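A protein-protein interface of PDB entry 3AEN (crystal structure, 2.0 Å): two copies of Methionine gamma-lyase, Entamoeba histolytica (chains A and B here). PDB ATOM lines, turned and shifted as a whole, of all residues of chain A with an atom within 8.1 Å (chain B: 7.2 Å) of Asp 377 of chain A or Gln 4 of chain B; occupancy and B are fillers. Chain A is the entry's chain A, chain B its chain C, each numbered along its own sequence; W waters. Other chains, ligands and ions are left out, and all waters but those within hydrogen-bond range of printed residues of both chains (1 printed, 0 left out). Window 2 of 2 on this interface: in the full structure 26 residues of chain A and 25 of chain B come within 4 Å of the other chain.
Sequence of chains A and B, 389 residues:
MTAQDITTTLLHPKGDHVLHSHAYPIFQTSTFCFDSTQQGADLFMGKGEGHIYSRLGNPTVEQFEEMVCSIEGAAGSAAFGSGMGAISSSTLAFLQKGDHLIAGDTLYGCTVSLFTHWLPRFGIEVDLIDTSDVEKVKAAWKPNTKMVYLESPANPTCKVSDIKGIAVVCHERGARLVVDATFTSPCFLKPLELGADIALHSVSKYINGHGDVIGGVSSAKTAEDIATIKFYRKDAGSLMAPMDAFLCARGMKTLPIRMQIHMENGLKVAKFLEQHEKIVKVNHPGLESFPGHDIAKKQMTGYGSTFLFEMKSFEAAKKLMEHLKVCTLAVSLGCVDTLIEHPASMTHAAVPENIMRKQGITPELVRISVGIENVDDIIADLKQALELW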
ATOM      1  N   VAL A 269     -13.841  10.846 -30.300  1.00  0.00           N
ATOM      2  CA  VAL A 269     -14.481  11.293 -29.058  1.00  0.00           C
ATOM      3  C   VAL A 269     -14.149  12.769 -28.812  1.00  0.00           C
ATOM      4  O   VAL A 269     -15.033  13.551 -28.493  1.00  0.00           O
ATOM      5  CB  VAL A 269     -14.088  10.407 -27.846  1.00  0.00           C
ATOM      6  CG1 VAL A 269     -14.572  11.029 -26.521  1.00  0.00           C
ATOM      7  CG2 VAL A 269     -14.678   8.979 -28.043  1.00  0.00           C
ATOM      8  N   LEU A 324     -22.710   7.686 -16.561  1.00  0.00           N
ATOM      9  CA  LEU A 324     -22.174   6.912 -17.688  1.00  0.00           C
ATOM     10  C   LEU A 324     -22.373   5.411 -17.463  1.00  0.00           C
ATOM     11  O   LEU A 324     -22.349   4.942 -16.336  1.00  0.00           O
ATOM     12  CB  LEU A 324     -20.691   7.265 -17.867  1.00  0.00           C
ATOM     13  CG  LEU A 324     -20.488   8.721 -18.254  1.00  0.00           C
ATOM     14  CD1 LEU A 324     -19.007   9.211 -18.096  1.00  0.00           C
ATOM     15  CD2 LEU A 324     -21.051   8.971 -19.673  1.00  0.00           C
ATOM     16  N   LYS A 325     -22.599   4.646 -18.519  1.00  0.00           N
ATOM     17  CA  LYS A 325     -22.811   3.206 -18.349  1.00  0.00           C
ATOM     18  C   LYS A 325     -21.695   2.377 -18.938  1.00  0.00           C
ATOM     19  O   LYS A 325     -21.504   1.232 -18.568  1.00  0.00           O
ATOM     20  CB  LYS A 325     -24.190   2.775 -18.891  1.00  0.00           C
ATOM     21  CG  LYS A 325     -25.335   3.113 -17.921  1.00  0.00           C
ATOM     22  CD  LYS A 325     -26.018   4.432 -18.328  1.00  0.00           C
ATOM     23  CE  LYS A 325     -27.152   4.863 -17.376  1.00  0.00           C
ATOM     24  NZ  LYS A 325     -26.756   5.791 -16.237  1.00  0.00           N
ATOM     25  N   VAL A 326     -20.957   2.967 -19.862  1.00  0.00           N
ATOM     26  CA  VAL A 326     -19.854   2.317 -20.487  1.00  0.00           C
ATOM     27  C   VAL A 326     -18.566   2.837 -19.793  1.00  0.00           C
ATOM     28  O   VAL A 326     -17.809   2.029 -19.229  1.00  0.00           O
ATOM     29  CB  VAL A 326     -19.905   2.538 -22.044  1.00  0.00           C
ATOM     30  CG1 VAL A 326     -18.784   1.811 -22.762  1.00  0.00           C
ATOM     31  CG2 VAL A 326     -21.274   2.022 -22.607  1.00  0.00           C
ATOM     32  N   CYS A 327     -18.345   4.149 -19.752  1.00  0.00           N
ATOM     33  CA  CYS A 327     -17.169   4.696 -19.088  1.00  0.00           C
ATOM     34  C   CYS A 327     -17.190   4.299 -17.601  1.00  0.00           C
ATOM     35  O   CYS A 327     -18.271   4.203 -17.016  1.00  0.00           O
ATOM     36  CB  CYS A 327     -17.153   6.206 -19.251  1.00  0.00           C
ATOM     37  SG  CYS A 327     -17.363   6.728 -20.986  1.00  0.00           S
ATOM     38  N   THR A 338     -12.942   2.115 -21.205  1.00  0.00           N
ATOM     39  CA  THR A 338     -12.870   3.550 -21.038  1.00  0.00           C
ATOM     40  C   THR A 338     -12.997   3.943 -19.542  1.00  0.00           C
ATOM     41  O   THR A 338     -13.885   3.438 -18.826  1.00  0.00           O
ATOM     42  CB  THR A 338     -13.928   4.242 -21.913  1.00  0.00           C
ATOM     43  OG1 THR A 338     -13.600   4.006 -23.294  1.00  0.00           O
ATOM     44  CG2 THR A 338     -13.980   5.738 -21.664  1.00  0.00           C
ATOM     45  N   GLU A 373     -13.416  -0.094 -26.931  1.00  0.00           N
ATOM     46  CA  GLU A 373     -14.850  -0.324 -27.218  1.00  0.00           C
ATOM     47  C   GLU A 373     -15.217   0.318 -28.560  1.00  0.00           C
ATOM     48  O   GLU A 373     -14.534   1.220 -29.039  1.00  0.00           O
ATOM     49  CB  GLU A 373     -15.764   0.348 -26.156  1.00  0.00           C
ATOM     50  CG  GLU A 373     -15.642  -0.163 -24.698  1.00  0.00           C
ATOM     51  CD  GLU A 373     -14.749   0.745 -23.874  1.00  0.00           C
ATOM     52  OE1 GLU A 373     -14.871   0.773 -22.634  1.00  0.00           O
ATOM     53  OE2 GLU A 373     -13.928   1.459 -24.490  1.00  0.00           O
ATOM     54  N   ASN A 374     -16.325  -0.099 -29.142  1.00  0.00           N
ATOM     55  CA  ASN A 374     -16.790   0.541 -30.351  1.00  0.00           C
ATOM     56  C   ASN A 374     -17.040   2.029 -30.104  1.00  0.00           C
ATOM     57  O   ASN A 374     -17.698   2.411 -29.122  1.00  0.00           O
ATOM     58  CB  ASN A 374     -18.086  -0.103 -30.811  1.00  0.00           C
ATOM     59  CG  ASN A 374     -18.627   0.541 -32.080  1.00  0.00           C
ATOM     60  OD1 ASN A 374     -18.383   0.059 -33.194  1.00  0.00           O
ATOM     61  ND2 ASN A 374     -19.364   1.607 -31.921  1.00  0.00           N
ATOM     62  N   VAL A 375     -16.515   2.868 -30.997  1.00  0.00           N
ATOM     63  CA  VAL A 375     -16.457   4.300 -30.743  1.00  0.00           C
ATOM     64  C   VAL A 375     -17.859   4.931 -30.683  1.00  0.00           C
ATOM     65  O   VAL A 375     -18.106   5.849 -29.903  1.00  0.00           O
ATOM     66  CB  VAL A 375     -15.514   5.055 -31.737  1.00  0.00           C
ATOM     67  CG1 VAL A 375     -16.080   5.032 -33.184  1.00  0.00           C
ATOM     68  CG2 VAL A 375     -15.253   6.472 -31.222  1.00  0.00           C
ATOM     69  N   ASP A 376     -18.771   4.409 -31.497  1.00  0.00           N
ATOM     70  CA  ASP A 376     -20.159   4.844 -31.446  1.00  0.00           C
ATOM     71  C   ASP A 376     -20.858   4.546 -30.103  1.00  0.00           C
ATOM     72  O   ASP A 376     -21.682   5.335 -29.662  1.00  0.00           O
ATOM     73  CB  ASP A 376     -20.909   4.215 -32.632  1.00  0.00           C
ATOM     74  CG  ASP A 376     -20.361   4.703 -33.978  1.00  0.00           C
ATOM     75  OD1 ASP A 376     -20.414   3.940 -34.948  1.00  0.00           O
ATOM     76  OD2 ASP A 376     -19.880   5.869 -34.052  1.00  0.00           O
ATOM     77  N   ASP A 377     -20.532   3.406 -29.471  1.00  0.00           N
ATOM     78  CA  ASP A 377     -21.078   3.067 -28.144  1.00  0.00           C
ATOM     79  C   ASP A 377     -20.548   4.038 -27.077  1.00  0.00           C
ATOM     80  O   ASP A 377     -21.302   4.448 -26.183  1.00  0.00           O
ATOM     81  CB  ASP A 377     -20.703   1.616 -27.740  1.00  0.00           C
ATOM     82  CG  ASP A 377     -21.377   0.563 -28.615  1.00  0.00           C
ATOM     83  OD1 ASP A 377     -22.442   0.860 -29.157  1.00  0.00           O
ATOM     84  OD2 ASP A 377     -20.853  -0.558 -28.756  1.00  0.00           O
ATOM     85  N   ILE A 378     -19.252   4.365 -27.148  1.00  0.00           N
ATOM     86  CA  ILE A 378     -18.665   5.405 -26.251  1.00  0.00           C
ATOM     87  C   ILE A 378     -19.307   6.788 -26.435  1.00  0.00           C
ATOM     88  O   ILE A 378     -19.696   7.440 -25.468  1.00  0.00           O
ATOM     89  CB  ILE A 378     -17.138   5.543 -26.392  1.00  0.00           C
ATOM     90  CG1 ILE A 378     -16.425   4.203 -26.149  1.00  0.00           C
ATOM     91  CG2 ILE A 378     -16.588   6.631 -25.420  1.00  0.00           C
ATOM     92  CD1 ILE A 378     -15.002   4.171 -26.813  1.00  0.00           C
ATOM     93  N   ILE A 379     -19.396   7.242 -27.673  1.00  0.00           N
ATOM     94  CA  ILE A 379     -20.042   8.512 -27.952  1.00  0.00           C
ATOM     95  C   ILE A 379     -21.517   8.532 -27.511  1.00  0.00           C
ATOM     96  O   ILE A 379     -21.934   9.504 -26.908  1.00  0.00           O
ATOM     97  CB  ILE A 379     -19.827   8.963 -29.436  1.00  0.00           C
ATOM     98  CG1 ILE A 379     -18.370   9.410 -29.645  1.00  0.00           C
ATOM     99  CG2 ILE A 379     -20.843  10.100 -29.859  1.00  0.00           C
ATOM    100  CD1 ILE A 379     -17.939   9.413 -31.147  1.00  0.00           C
ATOM    101  N   ALA A 380     -22.276   7.449 -27.734  1.00  0.00           N
ATOM    102  CA  ALA A 380     -23.691   7.421 -27.333  1.00  0.00           C
ATOM    103  C   ALA A 380     -23.833   7.506 -25.802  1.00  0.00           C
ATOM    104  O   ALA A 380     -24.798   8.071 -25.296  1.00  0.00           O
ATOM    105  CB  ALA A 380     -24.442   6.159 -27.901  1.00  0.00           C
ATOM    106  N   ASP A 381     -22.878   6.923 -25.078  1.00  0.00           N
ATOM    107  CA  ASP A 381     -22.906   6.915 -23.616  1.00  0.00           C
ATOM    108  C   ASP A 381     -22.641   8.351 -23.122  1.00  0.00           C
ATOM    109  O   ASP A 381     -23.320   8.836 -22.202  1.00  0.00           O
ATOM    110  CB  ASP A 381     -21.809   5.938 -23.099  1.00  0.00           C
ATOM    111  CG  ASP A 381     -21.828   5.736 -21.568  1.00  0.00           C
ATOM    112  OD1 ASP A 381     -22.926   5.623 -20.953  1.00  0.00           O
ATOM    113  OD2 ASP A 381     -20.717   5.696 -20.980  1.00  0.00           O
ATOM    114  N   LEU A 382     -21.642   9.013 -23.690  1.00  0.00           N
ATOM    115  CA  LEU A 382     -21.358  10.412 -23.343  1.00  0.00           C
ATOM    116  C   LEU A 382     -22.529  11.307 -23.715  1.00  0.00           C
ATOM    117  O   LEU A 382     -22.948  12.177 -22.943  1.00  0.00           O
ATOM    118  CB  LEU A 382     -20.060  10.923 -24.025  1.00  0.00           C
ATOM    119  CG  LEU A 382     -18.775  10.286 -23.484  1.00  0.00           C
ATOM    120  CD1 LEU A 382     -17.607  10.530 -24.442  1.00  0.00           C
ATOM    121  CD2 LEU A 382     -18.423  10.743 -22.063  1.00  0.00           C
ATOM    122  N   LYS A 383     -23.075  11.088 -24.901  1.00  0.00           N
ATOM    123  CA  LYS A 383     -24.164  11.947 -25.372  1.00  0.00           C
ATOM    124  C   LYS A 383     -25.419  11.840 -24.474  1.00  0.00           C
ATOM    125  O   LYS A 383     -26.040  12.853 -24.163  1.00  0.00           O
ATOM    126  CB  LYS A 383     -24.510  11.557 -26.798  1.00  0.00           C
ATOM    127  CG  LYS A 383     -25.520  12.471 -27.462  1.00  0.00           C
ATOM    128  CD  LYS A 383     -25.521  12.150 -28.964  1.00  0.00           C
ATOM    129  CE  LYS A 383     -26.602  12.911 -29.712  1.00  0.00           C
ATOM    130  NZ  LYS A 383     -27.680  11.941 -29.962  1.00  0.00           N
ATOM    131  N   GLN A 384     -25.803  10.614 -24.084  1.00  0.00           N
ATOM    132  CA  GLN A 384     -26.954  10.454 -23.205  1.00  0.00           C
ATOM    133  C   GLN A 384     -26.761  11.158 -21.849  1.00  0.00           C
ATOM    134  O   GLN A 384     -27.679  11.814 -21.356  1.00  0.00           O
ATOM    135  CB  GLN A 384     -27.446   8.986 -23.099  1.00  0.00           C
ATOM    136  CG  GLN A 384     -26.399   7.962 -22.499  1.00  0.00           C
ATOM    137  CD  GLN A 384     -26.467   7.881 -20.956  1.00  0.00           C
ATOM    138  OE1 GLN A 384     -27.579   7.923 -20.383  1.00  0.00           O
ATOM    139  NE2 GLN A 384     -25.295   7.760 -20.283  1.00  0.00           N
ATOM    140  N   ALA B   3     -27.997  -1.293 -31.055  1.00  0.00           N
ATOM    141  CA  ALA B   3     -27.384  -2.541 -30.501  1.00  0.00           C
ATOM    142  C   ALA B   3     -25.888  -2.351 -30.209  1.00  0.00           C
ATOM    143  O   ALA B   3     -25.098  -2.016 -31.100  1.00  0.00           O
ATOM    144  CB  ALA B   3     -27.588  -3.696 -31.443  1.00  0.00           C
ATOM    145  N   GLN B   4     -25.518  -2.557 -28.952  1.00  0.00           N
ATOM    146  CA  GLN B   4     -24.162  -2.392 -28.481  1.00  0.00           C
ATOM    147  C   GLN B   4     -23.212  -3.415 -29.153  1.00  0.00           C
ATOM    148  O   GLN B   4     -23.532  -4.602 -29.257  1.00  0.00           O
ATOM    149  CB  GLN B   4     -24.189  -2.597 -26.975  1.00  0.00           C
ATOM    150  CG  GLN B   4     -22.884  -2.608 -26.315  1.00  0.00           C
ATOM    151  CD  GLN B   4     -23.027  -2.668 -24.816  1.00  0.00           C
ATOM    152  OE1 GLN B   4     -23.436  -1.697 -24.181  1.00  0.00           O
ATOM    153  NE2 GLN B   4     -22.714  -3.830 -24.237  1.00  0.00           N
ATOM    154  N   ASP B   5     -22.058  -2.939 -29.613  1.00  0.00           N
ATOM    155  CA  ASP B   5     -21.103  -3.807 -30.311  1.00  0.00           C
ATOM    156  C   ASP B   5     -20.514  -4.892 -29.381  1.00  0.00           C
ATOM    157  O   ASP B   5     -20.370  -4.678 -28.160  1.00  0.00           O
ATOM    158  CB  ASP B   5     -19.977  -2.975 -30.894  1.00  0.00           C
ATOM    159  CG  ASP B   5     -19.209  -3.719 -31.936  1.00  0.00           C
ATOM    160  OD1 ASP B   5     -19.687  -3.746 -33.071  1.00  0.00           O
ATOM    161  OD2 ASP B   5     -18.141  -4.290 -31.621  1.00  0.00           O
ATOM    162  N   ILE B   6     -20.201  -6.067 -29.958  1.00  0.00           N
ATOM    163  CA  ILE B   6     -19.551  -7.148 -29.197  1.00  0.00           C
ATOM    164  C   ILE B   6     -18.231  -6.685 -28.515  1.00  0.00           C
ATOM    165  O   ILE B   6     -17.898  -7.101 -27.400  1.00  0.00           O
ATOM    166  CB  ILE B   6     -19.330  -8.408 -30.099  1.00  0.00           C
ATOM    167  CG1 ILE B   6     -18.897  -9.601 -29.256  1.00  0.00           C
ATOM    168  CG2 ILE B   6     -18.353  -8.099 -31.288  1.00  0.00           C
ATOM    169  CD1 ILE B   6     -19.819  -9.882 -28.032  1.00  0.00           C
ATOM    170  N   THR B   7     -17.493  -5.805 -29.182  1.00  0.00           N
ATOM    171  CA  THR B   7     -16.303  -5.232 -28.588  1.00  0.00           C
ATOM    172  C   THR B   7     -16.660  -4.647 -27.202  1.00  0.00           C
ATOM    173  O   THR B   7     -16.057  -5.019 -26.190  1.00  0.00           O
ATOM    174  CB  THR B   7     -15.689  -4.186 -29.569  1.00  0.00           C
ATOM    175  OG1 THR B   7     -15.455  -4.841 -30.841  1.00  0.00           O
ATOM    176  CG2 THR B   7     -14.362  -3.717 -29.106  1.00  0.00           C
ATOM    177  N   THR B   8     -17.706  -3.803 -27.148  1.00  0.00           N
ATOM    178  CA  THR B   8     -18.128  -3.166 -25.906  1.00  0.00           C
ATOM    179  C   THR B   8     -18.649  -4.162 -24.870  1.00  0.00           C
ATOM    180  O   THR B   8     -18.271  -4.111 -23.717  1.00  0.00           O
ATOM    181  CB  THR B   8     -19.255  -2.131 -26.225  1.00  0.00           C
ATOM    182  OG1 THR B   8     -18.802  -1.294 -27.306  1.00  0.00           O
ATOM    183  CG2 THR B   8     -19.589  -1.282 -25.002  1.00  0.00           C
ATOM    184  N   THR B   9     -19.511  -5.075 -25.300  1.00  0.00           N
ATOM    185  CA  THR B   9     -20.057  -6.129 -24.442  1.00  0.00           C
ATOM    186  C   THR B   9     -18.976  -6.943 -23.728  1.00  0.00           C
ATOM    187  O   THR B   9     -19.059  -7.183 -22.510  1.00  0.00           O
ATOM    188  CB  THR B   9     -20.891  -7.058 -25.329  1.00  0.00           C
ATOM    189  OG1 THR B   9     -22.024  -6.321 -25.700  1.00  0.00           O
ATOM    190  CG2 THR B   9     -21.328  -8.349 -24.623  1.00  0.00           C
ATOM    191  N   LEU B  10     -17.960  -7.352 -24.466  1.00  0.00           N
ATOM    192  CA  LEU B  10     -16.886  -8.158 -23.855  1.00  0.00           C
ATOM    193  C   LEU B  10     -16.031  -7.357 -22.845  1.00  0.00           C
ATOM    194  O   LEU B  10     -15.526  -7.916 -21.858  1.00  0.00           O
ATOM    195  CB  LEU B  10     -16.010  -8.750 -24.961  1.00  0.00           C
ATOM    196  CG  LEU B  10     -16.639  -9.885 -25.776  1.00  0.00           C
ATOM    197  CD1 LEU B  10     -15.684 -10.277 -26.875  1.00  0.00           C
ATOM    198  CD2 LEU B  10     -16.959 -11.120 -24.876  1.00  0.00           C
ATOM    199  N   HIS B  12     -17.332  -4.949 -21.046  1.00  0.00           N
ATOM    200  CA  HIS B  12     -18.317  -4.544 -19.993  1.00  0.00           C
ATOM    201  C   HIS B  12     -19.247  -5.685 -19.573  1.00  0.00           C
ATOM    202  O   HIS B  12     -20.444  -5.601 -19.785  1.00  0.00           O
ATOM    203  CB  HIS B  12     -19.096  -3.285 -20.424  1.00  0.00           C
ATOM    204  CG  HIS B  12     -18.183  -2.128 -20.653  1.00  0.00           C
ATOM    205  ND1 HIS B  12     -17.710  -1.348 -19.616  1.00  0.00           N
ATOM    206  CD2 HIS B  12     -17.532  -1.712 -21.769  1.00  0.00           C
ATOM    207  CE1 HIS B  12     -16.830  -0.482 -20.089  1.00  0.00           C
ATOM    208  NE2 HIS B  12     -16.708  -0.675 -21.393  1.00  0.00           N
HETATM  209  O   HOH W   1     -22.810  -0.277 -31.421  1.00  0.00           O
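No position is printed for both chains.
ND2 of Asn 374 of chain A lies close to N of Asp 376 of chain A (2.9 Å). N of Val 326 of chain A lies within hydrogen-bond range of OD2 of Asp 381 of chain A, at 3.0 Å. NE2 of Gln 4 of chain B lies within hydrogen-bond range of OG1 of Thr 9 of chain B, at 3.0 Å. The side-chain carboxylate (OD2) of Asp 5 of chain B sits at hydrogen-bond distance from the side-chain hydroxyl (OG1) of Thr 7 of chain B. O of Asp 5 of chain B lies within hydrogen-bond range of OG1 of Thr 9 of chain B, 3.4 Å away. The backbone NH of Thr 338 of chain A sits at hydrogen-bond distance from the side-chain carboxylate of Glu 373 of chain A, 2.8 Å away.
Among the printed residues, pairs that only touch across the chains: Val 326 of chain A with Thr 8 of chain B (3.9 Å), Glu 373 of chain A with Thr 7 of chain B (3.9 Å), Glu 373 of chain A with Thr 8 of chain B (3.6 Å), Asn 374 of chain A with Asp 5 of chain B (3.4 Å) and Asp 377 of chain A with Gln 4 of chain B (3.7 Å).
Of the 9 printed residues of chain B, 5 touch a printed residue of chain A. Hydrophobic or aromatic side chains of chain B within 4 Å of the printed part of chain A: His 12. Along chain B the printed residues that touch a printed residue of chain A span positions 4 to 12. Of the 18 printed residues of chain A, 4 touch a printed residue of chain B. Among the printed residues, 10 pairs touch across the chains. Among the printed residues, no Asp or Glu carboxylate lies within 4 Å of a Lys or Arg side-chain nitrogen of the other chain.
Water W1 lies within hydrogen-bond range of the side-chain carboxylate (OD1) of Asp 377 of chain A (2.6 Å), the backbone carbonyl oxygen (O) of Ala 3 of chain B (2.9 Å) and the backbone NH (N) of Asp 5 of chain B (3.3 Å).
Of chain B, only Gln 4 (3.7 Å), Asp 5 (2.8 Å) and Thr 8 (2.6 Å) come within 4 Å of Asp 377 of chain A. Gln 4 of chain B touches one residue of chain A. No residue of chain A comes within 4 Å of Ala 3 of chain B. Printed residues of chain B within 4 Å of Val 326 of chain A: Thr 8 and His 12. Of the printed residues of chain A, Asp 5 of chain B touches Asn 374 (3.4 Å) and Asp 377 (2.8 Å). Of the printed residues of chain A, His 12 of chain B touches Val 326 (2.8 Å) and Glu 373 (2.6 Å). Of the printed residues of chain A, Thr 7 of chain B touches Glu 373 (3.9 Å). Printed residues of chain B within 4 Å of Asn 374 of chain A: Asp 5 and Thr 8. The nearest residue of chain A that does not touch Gln 4 of chain B is Val 326 of chain A (4.6 Å).
OD2 of Asp 377 of chain A sits at hydrogen-bond distance from N of Asp 5 of chain B (2.8 Å). The backbone carbonyl oxygen (O) of Val 326 of chain A sits close to a ring nitrogen (ND1) of His 12 of chain B, at 3.4 Å. A ring nitrogen (NE2) of His 12 of chain B sits at hydrogen-bond distance from the side-chain carboxylate (OE1) of Glu 373 of chain A. OD2 of Asp 377 of chain A sits at hydrogen-bond distance from OG1 of Thr 8 of chain B, at 2.6 Å. The side-chain hydroxyl of Thr 8 of chain B is in hydrogen-bond range of the backbone NH of Asn 374 of chain A.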
